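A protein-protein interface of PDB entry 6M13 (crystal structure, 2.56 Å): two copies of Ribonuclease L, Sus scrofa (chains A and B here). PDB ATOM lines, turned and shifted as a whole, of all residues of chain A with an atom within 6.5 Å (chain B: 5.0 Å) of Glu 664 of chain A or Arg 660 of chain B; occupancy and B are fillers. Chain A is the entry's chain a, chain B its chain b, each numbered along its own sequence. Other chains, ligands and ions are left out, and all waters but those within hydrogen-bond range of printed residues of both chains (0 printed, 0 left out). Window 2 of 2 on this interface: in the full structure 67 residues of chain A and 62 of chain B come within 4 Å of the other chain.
The backbone carbonyl oxygen (O) of Glu 664 of chain B is in hydrogen-bond range of the side-chain amide nitrogen (ND2) of Asn 583 of chain A (3.1 Å). NH1 of Arg 660 of chain A lies within salt-bridge range of OE1 of Glu 664 of chain B, 2.9 Å away. The side-chain amide nitrogen (ND2) of Asn 583 of chain B is in hydrogen-bond range of the backbone carbonyl oxygen (O) of Glu 664 of chain A (3.1 Å). NH2 of Arg 660 of chain B lies within salt-bridge range of OE1 of Glu 664 of chain A, at 2.7 Å. The side-chain carboxylate of Glu 668 of chain A is in salt-bridge range of the side-chain amino group of Lys 588 of chain B (2.7 Å).
NH2 of Arg 579 of chain A is in salt-bridge range of OE2 of Glu 664 of chain A, 3.2 Å away. The side-chain amide oxygen (OD1) of Asn 583 of chain A lies within hydrogen-bond range of the guanidinium group (NH1) of Arg 660 of chain A (2.8 Å). The guanidinium group of Arg 660 of chain A sits at hydrogen-bond distance from the side-chain amide oxygen of Asn 661 of chain A (3.0 Å). The side-chain carboxylate of Glu 668 of chain A lies within hydrogen-bond range of a ring nitrogen (ND1) of His 665 of chain A, at 2.9 Å. NH2 of Arg 579 of chain B is in salt-bridge range of OE2 of Glu 664 of chain B (3.1 Å). The side-chain amide oxygen (OD1) of Asn 583 of chain B lies within hydrogen-bond range of the guanidinium group (NE) of Arg 660 of chain B (2.6 Å).
Among the printed residues, merely in contact across the chains: Glu 664 of chain A with Lys 588 of chain B and Glu 664 of chain A with Glu 664 of chain B.
Of the printed residues of chain B, Glu 664 of chain A touches Asn 583 (3.1 Å), Lys 588 (3.5 Å), Arg 660 (2.7 Å) and Glu 664 (3.6 Å). Arg 660 of chain B touches just one residue of chain A: Glu 664. Of the printed residues of chain A, Lys 588 of chain B touches Glu 664 and Glu 668. Of the printed residues of chain B, Glu 668 of chain A touches Lys 588. Of the printed residues of chain B, Asn 583 of chain A touches Glu 664 (3.1 Å). Of the printed residues of chain A, Glu 664 of chain B touches Asn 583 (3.1 Å), Arg 660 (2.9 Å) and Glu 664 (3.6 Å). Gly 663 of chain A touches none of the printed residues of chain B. Arg 576 of chain A touches none of the printed residues of chain B. The nearest printed residue of chain B that does not touch Glu 664 of chain A is Arg 579 of chain B (6.1 Å). The nearest residue of chain A that does not touch Arg 660 of chain B is His 665 of chain A (4.2 Å).
Of the 14 printed residues of chain A, 4 touch a printed residue of chain B. Printed residues of chain A that touch a printed residue of chain B: Asn 583, Arg 660, Glu 664 and Glu 668. Of the 15 printed residues of chain B, 4 touch a printed residue of chain A. Along chain B the printed residues that touch a printed residue of chain A span positions 583 to 664. Among the printed residues, Asp or Glu carboxylates within 4 Å of a Lys or Arg side-chain nitrogen of the other chain: Arg 660 of chain A with Glu 664 of chain B (2.9 Å), Glu 664 of chain A with Arg 660 of chain B (2.7 Å) and Glu 668 of chain A with Lys 588 of chain B (2.7 Å).
Asn 583 of chain A touches Glu 664 of chain B, and with the chains exchanged Glu 664 of chain A touches Asn 583 of chain B. Arg 660 of chain A touches Glu 664 of chain B, and with the chains exchanged Glu 664 of chain A touches Arg 660 of chain B. Glu 664 of chain B touches its own counterpart, Glu 664 of chain A.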
ATOM      1  N   TYR A 575      -6.185 -23.141  17.763  1.00  0.00           N
ATOM      2  CA  TYR A 575      -7.013 -21.991  17.348  1.00  0.00           C
ATOM      3  C   TYR A 575      -6.778 -21.561  15.872  1.00  0.00           C
ATOM      4  O   TYR A 575      -7.716 -21.340  15.128  1.00  0.00           O
ATOM      5  CB  TYR A 575      -6.750 -20.849  18.287  1.00  0.00           C
ATOM      6  CG  TYR A 575      -7.493 -19.552  18.072  1.00  0.00           C
ATOM      7  CD1 TYR A 575      -8.871 -19.517  17.840  1.00  0.00           C
ATOM      8  CD2 TYR A 575      -6.814 -18.335  18.187  1.00  0.00           C
ATOM      9  CE1 TYR A 575      -9.539 -18.313  17.691  1.00  0.00           C
ATOM     10  CE2 TYR A 575      -7.470 -17.134  18.034  1.00  0.00           C
ATOM     11  CZ  TYR A 575      -8.822 -17.114  17.798  1.00  0.00           C
ATOM     12  OH  TYR A 575      -9.405 -15.881  17.652  1.00  0.00           O
ATOM     13  N   ARG A 576      -5.538 -21.560  15.446  1.00  0.00           N
ATOM     14  CA  ARG A 576      -5.221 -21.245  14.062  1.00  0.00           C
ATOM     15  C   ARG A 576      -5.809 -22.239  13.069  1.00  0.00           C
ATOM     16  O   ARG A 576      -6.245 -21.874  11.996  1.00  0.00           O
ATOM     17  CB  ARG A 576      -3.696 -21.205  13.906  1.00  0.00           C
ATOM     18  CG  ARG A 576      -3.181 -20.792  12.570  1.00  0.00           C
ATOM     19  CD  ARG A 576      -3.443 -19.334  12.315  1.00  0.00           C
ATOM     20  NE  ARG A 576      -4.723 -19.088  11.670  1.00  0.00           N
ATOM     21  CZ  ARG A 576      -5.226 -17.883  11.420  1.00  0.00           C
ATOM     22  NH1 ARG A 576      -4.578 -16.780  11.789  1.00  0.00           N
ATOM     23  NH2 ARG A 576      -6.408 -17.772  10.849  1.00  0.00           N
ATOM     24  N   ARG A 579      -9.622 -21.750  12.859  1.00  0.00           N
ATOM     25  CA  ARG A 579      -9.882 -20.556  12.066  1.00  0.00           C
ATOM     26  C   ARG A 579      -9.689 -20.807  10.581  1.00  0.00           C
ATOM     27  O   ARG A 579     -10.511 -20.358   9.772  1.00  0.00           O
ATOM     28  CB  ARG A 579      -8.997 -19.398  12.526  1.00  0.00           C
ATOM     29  CG  ARG A 579      -9.396 -18.846  13.895  1.00  0.00           C
ATOM     30  CD  ARG A 579      -8.329 -17.937  14.468  1.00  0.00           C
ATOM     31  NE  ARG A 579      -8.149 -16.744  13.660  1.00  0.00           N
ATOM     32  CZ  ARG A 579      -7.227 -15.816  13.888  1.00  0.00           C
ATOM     33  NH1 ARG A 579      -6.386 -15.940  14.919  1.00  0.00           N
ATOM     34  NH2 ARG A 579      -7.162 -14.760  13.082  1.00  0.00           N
ATOM     35  N   ASN A 583     -12.577 -20.926   7.349  1.00  0.00           N
ATOM     36  CA  ASN A 583     -12.470 -19.988   6.260  1.00  0.00           C
ATOM     37  C   ASN A 583     -12.598 -20.640   4.899  1.00  0.00           C
ATOM     38  O   ASN A 583     -12.476 -19.960   3.875  1.00  0.00           O
ATOM     39  CB  ASN A 583     -11.107 -19.261   6.330  1.00  0.00           C
ATOM     40  CG  ASN A 583     -11.072 -18.025   5.494  1.00  0.00           C
ATOM     41  OD1 ASN A 583     -11.883 -17.098   5.663  1.00  0.00           O
ATOM     42  ND2 ASN A 583     -10.193 -18.034   4.535  1.00  0.00           N
ATOM     43  N   ILE A 659     -15.842 -19.384  14.671  1.00  0.00           N
ATOM     44  CA  ILE A 659     -14.484 -19.209  15.177  1.00  0.00           C
ATOM     45  C   ILE A 659     -13.612 -18.407  14.207  1.00  0.00           C
ATOM     46  O   ILE A 659     -12.873 -17.522  14.629  1.00  0.00           O
ATOM     47  CB  ILE A 659     -13.851 -20.549  15.536  1.00  0.00           C
ATOM     48  CG1 ILE A 659     -14.579 -21.157  16.758  1.00  0.00           C
ATOM     49  CG2 ILE A 659     -12.391 -20.367  15.890  1.00  0.00           C
ATOM     50  CD1 ILE A 659     -14.335 -22.671  16.905  1.00  0.00           C
ATOM     51  N   ARG A 660     -13.742 -18.681  12.918  1.00  0.00           N
ATOM     52  CA  ARG A 660     -13.046 -17.911  11.921  1.00  0.00           C
ATOM     53  C   ARG A 660     -13.421 -16.430  11.981  1.00  0.00           C
ATOM     54  O   ARG A 660     -12.540 -15.571  11.890  1.00  0.00           O
ATOM     55  CB  ARG A 660     -13.330 -18.449  10.530  1.00  0.00           C
ATOM     56  CG  ARG A 660     -12.609 -17.670   9.426  1.00  0.00           C
ATOM     57  CD  ARG A 660     -13.494 -17.281   8.281  1.00  0.00           C
ATOM     58  NE  ARG A 660     -13.998 -15.924   8.452  1.00  0.00           N
ATOM     59  CZ  ARG A 660     -13.468 -14.808   7.948  1.00  0.00           C
ATOM     60  NH1 ARG A 660     -12.379 -14.803   7.211  1.00  0.00           N
ATOM     61  NH2 ARG A 660     -14.087 -13.661   8.162  1.00  0.00           N
ATOM     62  N   ASN A 661     -14.714 -16.137  12.113  1.00  0.00           N
ATOM     63  CA  ASN A 661     -15.200 -14.746  12.099  1.00  0.00           C
ATOM     64  C   ASN A 661     -14.725 -13.999  13.316  1.00  0.00           C
ATOM     65  O   ASN A 661     -14.199 -12.907  13.199  1.00  0.00           O
ATOM     66  CB  ASN A 661     -16.738 -14.674  12.000  1.00  0.00           C
ATOM     67  CG  ASN A 661     -17.245 -14.988  10.607  1.00  0.00           C
ATOM     68  OD1 ASN A 661     -16.518 -14.832   9.590  1.00  0.00           O
ATOM     69  ND2 ASN A 661     -18.494 -15.461  10.544  1.00  0.00           N
ATOM     70  N   LEU A 662     -14.911 -14.599  14.480  1.00  0.00           N
ATOM     71  CA  LEU A 662     -14.487 -13.971  15.725  1.00  0.00           C
ATOM     72  C   LEU A 662     -12.992 -13.701  15.702  1.00  0.00           C
ATOM     73  O   LEU A 662     -12.563 -12.643  16.141  1.00  0.00           O
ATOM     74  CB  LEU A 662     -14.850 -14.844  16.914  1.00  0.00           C
ATOM     75  CG  LEU A 662     -14.794 -14.171  18.289  1.00  0.00           C
ATOM     76  CD1 LEU A 662     -15.908 -14.709  19.187  1.00  0.00           C
ATOM     77  CD2 LEU A 662     -13.438 -14.353  18.962  1.00  0.00           C
ATOM     78  N   GLY A 663     -12.217 -14.654  15.170  1.00  0.00           N
ATOM     79  CA  GLY A 663     -10.781 -14.516  15.091  1.00  0.00           C
ATOM     80  C   GLY A 663     -10.352 -13.261  14.357  1.00  0.00           C
ATOM     81  O   GLY A 663      -9.403 -12.573  14.763  1.00  0.00           O
ATOM     82  N   GLU A 664     -11.059 -12.958  13.276  1.00  0.00           N
ATOM     83  CA  GLU A 664     -10.685 -11.838  12.409  1.00  0.00           C
ATOM     84  C   GLU A 664     -11.065 -10.475  13.000  1.00  0.00           C
ATOM     85  O   GLU A 664     -10.338  -9.494  12.798  1.00  0.00           O
ATOM     86  CB  GLU A 664     -11.280 -12.026  11.018  1.00  0.00           C
ATOM     87  CG  GLU A 664     -10.657 -13.193  10.249  1.00  0.00           C
ATOM     88  CD  GLU A 664      -9.165 -13.042   9.995  1.00  0.00           C
ATOM     89  OE1 GLU A 664      -8.707 -11.964   9.523  1.00  0.00           O
ATOM     90  OE2 GLU A 664      -8.435 -14.028  10.224  1.00  0.00           O
ATOM     91  N   HIS A 665     -12.164 -10.414  13.746  1.00  0.00           N
ATOM     92  CA  HIS A 665     -12.735  -9.117  14.155  1.00  0.00           C
ATOM     93  C   HIS A 665     -12.698  -8.829  15.656  1.00  0.00           C
ATOM     94  O   HIS A 665     -13.110  -7.754  16.080  1.00  0.00           O
ATOM     95  CB  HIS A 665     -14.175  -8.971  13.637  1.00  0.00           C
ATOM     96  CG  HIS A 665     -14.327  -9.277  12.180  1.00  0.00           C
ATOM     97  ND1 HIS A 665     -13.673  -8.556  11.202  1.00  0.00           N
ATOM     98  CD2 HIS A 665     -15.053 -10.223  11.530  1.00  0.00           C
ATOM     99  CE1 HIS A 665     -13.952  -9.075  10.018  1.00  0.00           C
ATOM    100  NE2 HIS A 665     -14.791 -10.082  10.187  1.00  0.00           N
ATOM    101  N   ILE A 666     -12.199  -9.782  16.443  1.00  0.00           N
ATOM    102  CA  ILE A 666     -12.223  -9.671  17.901  1.00  0.00           C
ATOM    103  C   ILE A 666     -11.505  -8.437  18.419  1.00  0.00           C
ATOM    104  O   ILE A 666     -11.915  -7.895  19.430  1.00  0.00           O
ATOM    105  CB  ILE A 666     -11.650 -10.952  18.588  1.00  0.00           C
ATOM    106  CG1 ILE A 666     -11.947 -10.994  20.092  1.00  0.00           C
ATOM    107  CG2 ILE A 666     -10.157 -11.096  18.349  1.00  0.00           C
ATOM    108  CD1 ILE A 666     -13.420 -11.009  20.403  1.00  0.00           C
ATOM    109  N   ASN A 667     -10.454  -7.995  17.740  1.00  0.00           N
ATOM    110  CA  ASN A 667      -9.630  -6.890  18.234  1.00  0.00           C
ATOM    111  C   ASN A 667     -10.101  -5.486  17.842  1.00  0.00           C
ATOM    112  O   ASN A 667      -9.510  -4.525  18.308  1.00  0.00           O
ATOM    113  CB  ASN A 667      -8.207  -7.080  17.753  1.00  0.00           C
ATOM    114  CG  ASN A 667      -7.540  -8.245  18.409  1.00  0.00           C
ATOM    115  OD1 ASN A 667      -7.399  -8.269  19.635  1.00  0.00           O
ATOM    116  ND2 ASN A 667      -7.113  -9.221  17.602  1.00  0.00           N
ATOM    117  N   GLU A 668     -11.157  -5.375  17.024  1.00  0.00           N
ATOM    118  CA  GLU A 668     -11.641  -4.069  16.580  1.00  0.00           C
ATOM    119  C   GLU A 668     -12.298  -3.311  17.740  1.00  0.00           C
ATOM    120  O   GLU A 668     -12.814  -3.928  18.701  1.00  0.00           O
ATOM    121  CB  GLU A 668     -12.594  -4.222  15.387  1.00  0.00           C
ATOM    122  CG  GLU A 668     -11.902  -4.756  14.134  1.00  0.00           C
ATOM    123  CD  GLU A 668     -12.890  -5.267  13.067  1.00  0.00           C
ATOM    124  OE1 GLU A 668     -14.066  -4.851  13.093  1.00  0.00           O
ATOM    125  OE2 GLU A 668     -12.524  -6.144  12.222  1.00  0.00           O
ATOM    126  N   LEU B 578       2.617 -11.035   7.489  1.00  0.00           N
ATOM    127  CA  LEU B 578       2.130  -9.865   6.753  1.00  0.00           C
ATOM    128  C   LEU B 578       0.611  -9.776   6.826  1.00  0.00           C
ATOM    129  O   LEU B 578       0.063  -8.689   6.958  1.00  0.00           O
ATOM    130  CB  LEU B 578       2.569  -9.901   5.293  1.00  0.00           C
ATOM    131  CG  LEU B 578       4.080  -9.921   5.063  1.00  0.00           C
ATOM    132  CD1 LEU B 578       4.407 -10.039   3.593  1.00  0.00           C
ATOM    133  CD2 LEU B 578       4.750  -8.714   5.666  1.00  0.00           C
ATOM    134  N   ARG B 579      -0.057 -10.920   6.756  1.00  0.00           N
ATOM    135  CA  ARG B 579      -1.501 -10.952   6.929  1.00  0.00           C
ATOM    136  C   ARG B 579      -1.935 -10.531   8.341  1.00  0.00           C
ATOM    137  O   ARG B 579      -2.900  -9.790   8.512  1.00  0.00           O
ATOM    138  CB  ARG B 579      -2.053 -12.356   6.604  1.00  0.00           C
ATOM    139  CG  ARG B 579      -1.978 -12.703   5.130  1.00  0.00           C
ATOM    140  CD  ARG B 579      -2.206 -14.171   4.884  1.00  0.00           C
ATOM    141  NE  ARG B 579      -3.565 -14.591   5.239  1.00  0.00           N
ATOM    142  CZ  ARG B 579      -3.987 -15.854   5.146  1.00  0.00           C
ATOM    143  NH1 ARG B 579      -3.145 -16.813   4.763  1.00  0.00           N
ATOM    144  NH2 ARG B 579      -5.230 -16.174   5.447  1.00  0.00           N
ATOM    145  N   GLY B 582      -1.374  -6.802   8.939  1.00  0.00           N
ATOM    146  CA  GLY B 582      -2.453  -6.164   8.181  1.00  0.00           C
ATOM    147  C   GLY B 582      -3.856  -6.259   8.738  1.00  0.00           C
ATOM    148  O   GLY B 582      -4.729  -5.544   8.272  1.00  0.00           O
ATOM    149  N   ASN B 583      -4.056  -7.087   9.760  1.00  0.00           N
ATOM    150  CA  ASN B 583      -5.355  -7.227  10.422  1.00  0.00           C
ATOM    151  C   ASN B 583      -5.443  -6.430  11.714  1.00  0.00           C
ATOM    152  O   ASN B 583      -6.474  -6.462  12.369  1.00  0.00           O
ATOM    153  CB  ASN B 583      -5.615  -8.702  10.736  1.00  0.00           C
ATOM    154  CG  ASN B 583      -7.056  -8.968  11.117  1.00  0.00           C
ATOM    155  OD1 ASN B 583      -7.926  -8.814  10.303  1.00  0.00           O
ATOM    156  ND2 ASN B 583      -7.311  -9.352  12.364  1.00  0.00           N
ATOM    157  N   LYS B 588      -6.678  -1.278   9.420  1.00  0.00           N
ATOM    158  CA  LYS B 588      -7.947  -1.347   8.693  1.00  0.00           C
ATOM    159  C   LYS B 588      -8.714  -0.023   8.723  1.00  0.00           C
ATOM    160  O   LYS B 588      -9.376   0.331   7.750  1.00  0.00           O
ATOM    161  CB  LYS B 588      -8.807  -2.500   9.221  1.00  0.00           C
ATOM    162  CG  LYS B 588      -8.142  -3.855   8.990  1.00  0.00           C
ATOM    163  CD  LYS B 588      -9.074  -5.008   9.330  1.00  0.00           C
ATOM    164  CE  LYS B 588      -9.185  -5.201  10.838  1.00  0.00           C
ATOM    165  NZ  LYS B 588     -10.073  -6.328  11.222  1.00  0.00           N
ATOM    166  N   LEU B 656      -0.404  -3.846   3.645  1.00  0.00           N
ATOM    167  CA  LEU B 656      -0.597  -4.956   4.567  1.00  0.00           C
ATOM    168  C   LEU B 656      -2.083  -5.252   4.730  1.00  0.00           C
ATOM    169  O   LEU B 656      -2.484  -6.411   4.835  1.00  0.00           O
ATOM    170  CB  LEU B 656       0.094  -4.683   5.898  1.00  0.00           C
ATOM    171  CG  LEU B 656       1.592  -4.377   5.794  1.00  0.00           C
ATOM    172  CD1 LEU B 656       2.208  -3.918   7.084  1.00  0.00           C
ATOM    173  CD2 LEU B 656       2.349  -5.562   5.277  1.00  0.00           C
ATOM    174  N   LYS B 657      -2.913  -4.213   4.721  1.00  0.00           N
ATOM    175  CA  LYS B 657      -4.377  -4.406   4.673  1.00  0.00           C
ATOM    176  C   LYS B 657      -4.757  -5.142   3.394  1.00  0.00           C
ATOM    177  O   LYS B 657      -5.612  -6.030   3.409  1.00  0.00           O
ATOM    178  CB  LYS B 657      -5.134  -3.081   4.754  1.00  0.00           C
ATOM    179  CG  LYS B 657      -6.576  -3.178   5.289  1.00  0.00           C
ATOM    180  CD  LYS B 657      -7.531  -2.114   4.725  1.00  0.00           C
ATOM    181  CE  LYS B 657      -6.906  -0.707   4.563  1.00  0.00           C
ATOM    182  NZ  LYS B 657      -7.857   0.378   4.191  1.00  0.00           N
ATOM    183  N   PHE B 658      -4.116  -4.769   2.291  1.00  0.00           N
ATOM    184  CA  PHE B 658      -4.345  -5.413   1.025  1.00  0.00           C
ATOM    185  C   PHE B 658      -4.032  -6.909   1.142  1.00  0.00           C
ATOM    186  O   PHE B 658      -4.834  -7.749   0.721  1.00  0.00           O
ATOM    187  CB  PHE B 658      -3.489  -4.757  -0.069  1.00  0.00           C
ATOM    188  CG  PHE B 658      -3.744  -5.308  -1.445  1.00  0.00           C
ATOM    189  CD1 PHE B 658      -4.739  -4.771  -2.256  1.00  0.00           C
ATOM    190  CD2 PHE B 658      -2.983  -6.359  -1.933  1.00  0.00           C
ATOM    191  CE1 PHE B 658      -4.954  -5.277  -3.522  1.00  0.00           C
ATOM    192  CE2 PHE B 658      -3.218  -6.884  -3.194  1.00  0.00           C
ATOM    193  CZ  PHE B 658      -4.197  -6.347  -3.982  1.00  0.00           C
ATOM    194  N   ILE B 659      -2.873  -7.222   1.729  1.00  0.00           N
ATOM    195  CA  ILE B 659      -2.421  -8.602   1.858  1.00  0.00           C
ATOM    196  C   ILE B 659      -3.318  -9.412   2.807  1.00  0.00           C
ATOM    197  O   ILE B 659      -3.675 -10.545   2.515  1.00  0.00           O
ATOM    198  CB  ILE B 659      -0.959  -8.664   2.266  1.00  0.00           C
ATOM    199  CG1 ILE B 659      -0.087  -8.132   1.111  1.00  0.00           C
ATOM    200  CG2 ILE B 659      -0.565 -10.114   2.531  1.00  0.00           C
ATOM    201  CD1 ILE B 659       1.362  -7.835   1.444  1.00  0.00           C
ATOM    202  N   ARG B 660      -3.715  -8.810   3.910  1.00  0.00           N
ATOM    203  CA  ARG B 660      -4.667  -9.442   4.797  1.00  0.00           C
ATOM    204  C   ARG B 660      -5.981  -9.763   4.113  1.00  0.00           C
ATOM    205  O   ARG B 660      -6.511 -10.856   4.300  1.00  0.00           O
ATOM    206  CB  ARG B 660      -4.906  -8.564   6.021  1.00  0.00           C
ATOM    207  CG  ARG B 660      -5.938  -9.089   6.992  1.00  0.00           C
ATOM    208  CD  ARG B 660      -7.298  -8.483   6.736  1.00  0.00           C
ATOM    209  NE  ARG B 660      -8.269  -8.993   7.682  1.00  0.00           N
ATOM    210  CZ  ARG B 660      -9.454  -9.521   7.394  1.00  0.00           C
ATOM    211  NH1 ARG B 660      -9.910  -9.618   6.159  1.00  0.00           N
ATOM    212  NH2 ARG B 660     -10.199  -9.989   8.387  1.00  0.00           N
ATOM    213  N   ASN B 661      -6.515  -8.805   3.346  1.00  0.00           N
ATOM    214  CA  ASN B 661      -7.840  -8.964   2.707  1.00  0.00           C
ATOM    215  C   ASN B 661      -7.806 -10.042   1.648  1.00  0.00           C
ATOM    216  O   ASN B 661      -8.659 -10.931   1.634  1.00  0.00           O
ATOM    217  CB  ASN B 661      -8.325  -7.658   2.083  1.00  0.00           C
ATOM    218  CG  ASN B 661      -8.821  -6.656   3.104  1.00  0.00           C
ATOM    219  OD1 ASN B 661      -9.252  -7.004   4.197  1.00  0.00           O
ATOM    220  ND2 ASN B 661      -8.779  -5.382   2.734  1.00  0.00           N
ATOM    221  N   LEU B 662      -6.793  -9.980   0.791  1.00  0.00           N
ATOM    222  CA  LEU B 662      -6.623 -10.989  -0.235  1.00  0.00           C
ATOM    223  C   LEU B 662      -6.481 -12.364   0.387  1.00  0.00           C
ATOM    224  O   LEU B 662      -7.027 -13.324  -0.134  1.00  0.00           O
ATOM    225  CB  LEU B 662      -5.403 -10.671  -1.088  1.00  0.00           C
ATOM    226  CG  LEU B 662      -5.290 -11.417  -2.418  1.00  0.00           C
ATOM    227  CD1 LEU B 662      -4.712 -10.478  -3.491  1.00  0.00           C
ATOM    228  CD2 LEU B 662      -4.453 -12.683  -2.279  1.00  0.00           C
ATOM    229  N   GLY B 663      -5.738 -12.460   1.493  1.00  0.00           N
ATOM    230  CA  GLY B 663      -5.497 -13.720   2.160  1.00  0.00           C
ATOM    231  C   GLY B 663      -6.782 -14.413   2.553  1.00  0.00           C
ATOM    232  O   GLY B 663      -6.912 -15.644   2.400  1.00  0.00           O
ATOM    233  N   GLU B 664      -7.744 -13.619   3.018  1.00  0.00           N
ATOM    234  CA  GLU B 664      -8.994 -14.165   3.528  1.00  0.00           C
ATOM    235  C   GLU B 664      -9.943 -14.628   2.434  1.00  0.00           C
ATOM    236  O   GLU B 664     -10.644 -15.648   2.611  1.00  0.00           O
ATOM    237  CB  GLU B 664      -9.668 -13.149   4.461  1.00  0.00           C
ATOM    238  CG  GLU B 664      -8.897 -12.864   5.754  1.00  0.00           C
ATOM    239  CD  GLU B 664      -8.556 -14.126   6.579  1.00  0.00           C
ATOM    240  OE1 GLU B 664      -9.504 -14.876   6.922  1.00  0.00           O
ATOM    241  OE2 GLU B 664      -7.343 -14.373   6.832  1.00  0.00           O
ATOM    242  N   HIS B 665      -9.944 -13.925   1.289  1.00  0.00           N
ATOM    243  CA  HIS B 665     -10.964 -14.169   0.257  1.00  0.00           C
ATOM    244  C   HIS B 665     -10.440 -14.739  -1.064  1.00  0.00           C
ATOM    245  O   HIS B 665     -11.209 -14.942  -1.994  1.00  0.00           O
ATOM    246  CB  HIS B 665     -11.705 -12.875  -0.012  1.00  0.00           C
ATOM    247  CG  HIS B 665     -12.301 -12.250   1.204  1.00  0.00           C
ATOM    248  ND1 HIS B 665     -13.226 -12.904   1.993  1.00  0.00           N
ATOM    249  CD2 HIS B 665     -12.155 -11.015   1.733  1.00  0.00           C
ATOM    250  CE1 HIS B 665     -13.632 -12.096   2.953  1.00  0.00           C
ATOM    251  NE2 HIS B 665     -12.998 -10.940   2.817  1.00  0.00           N
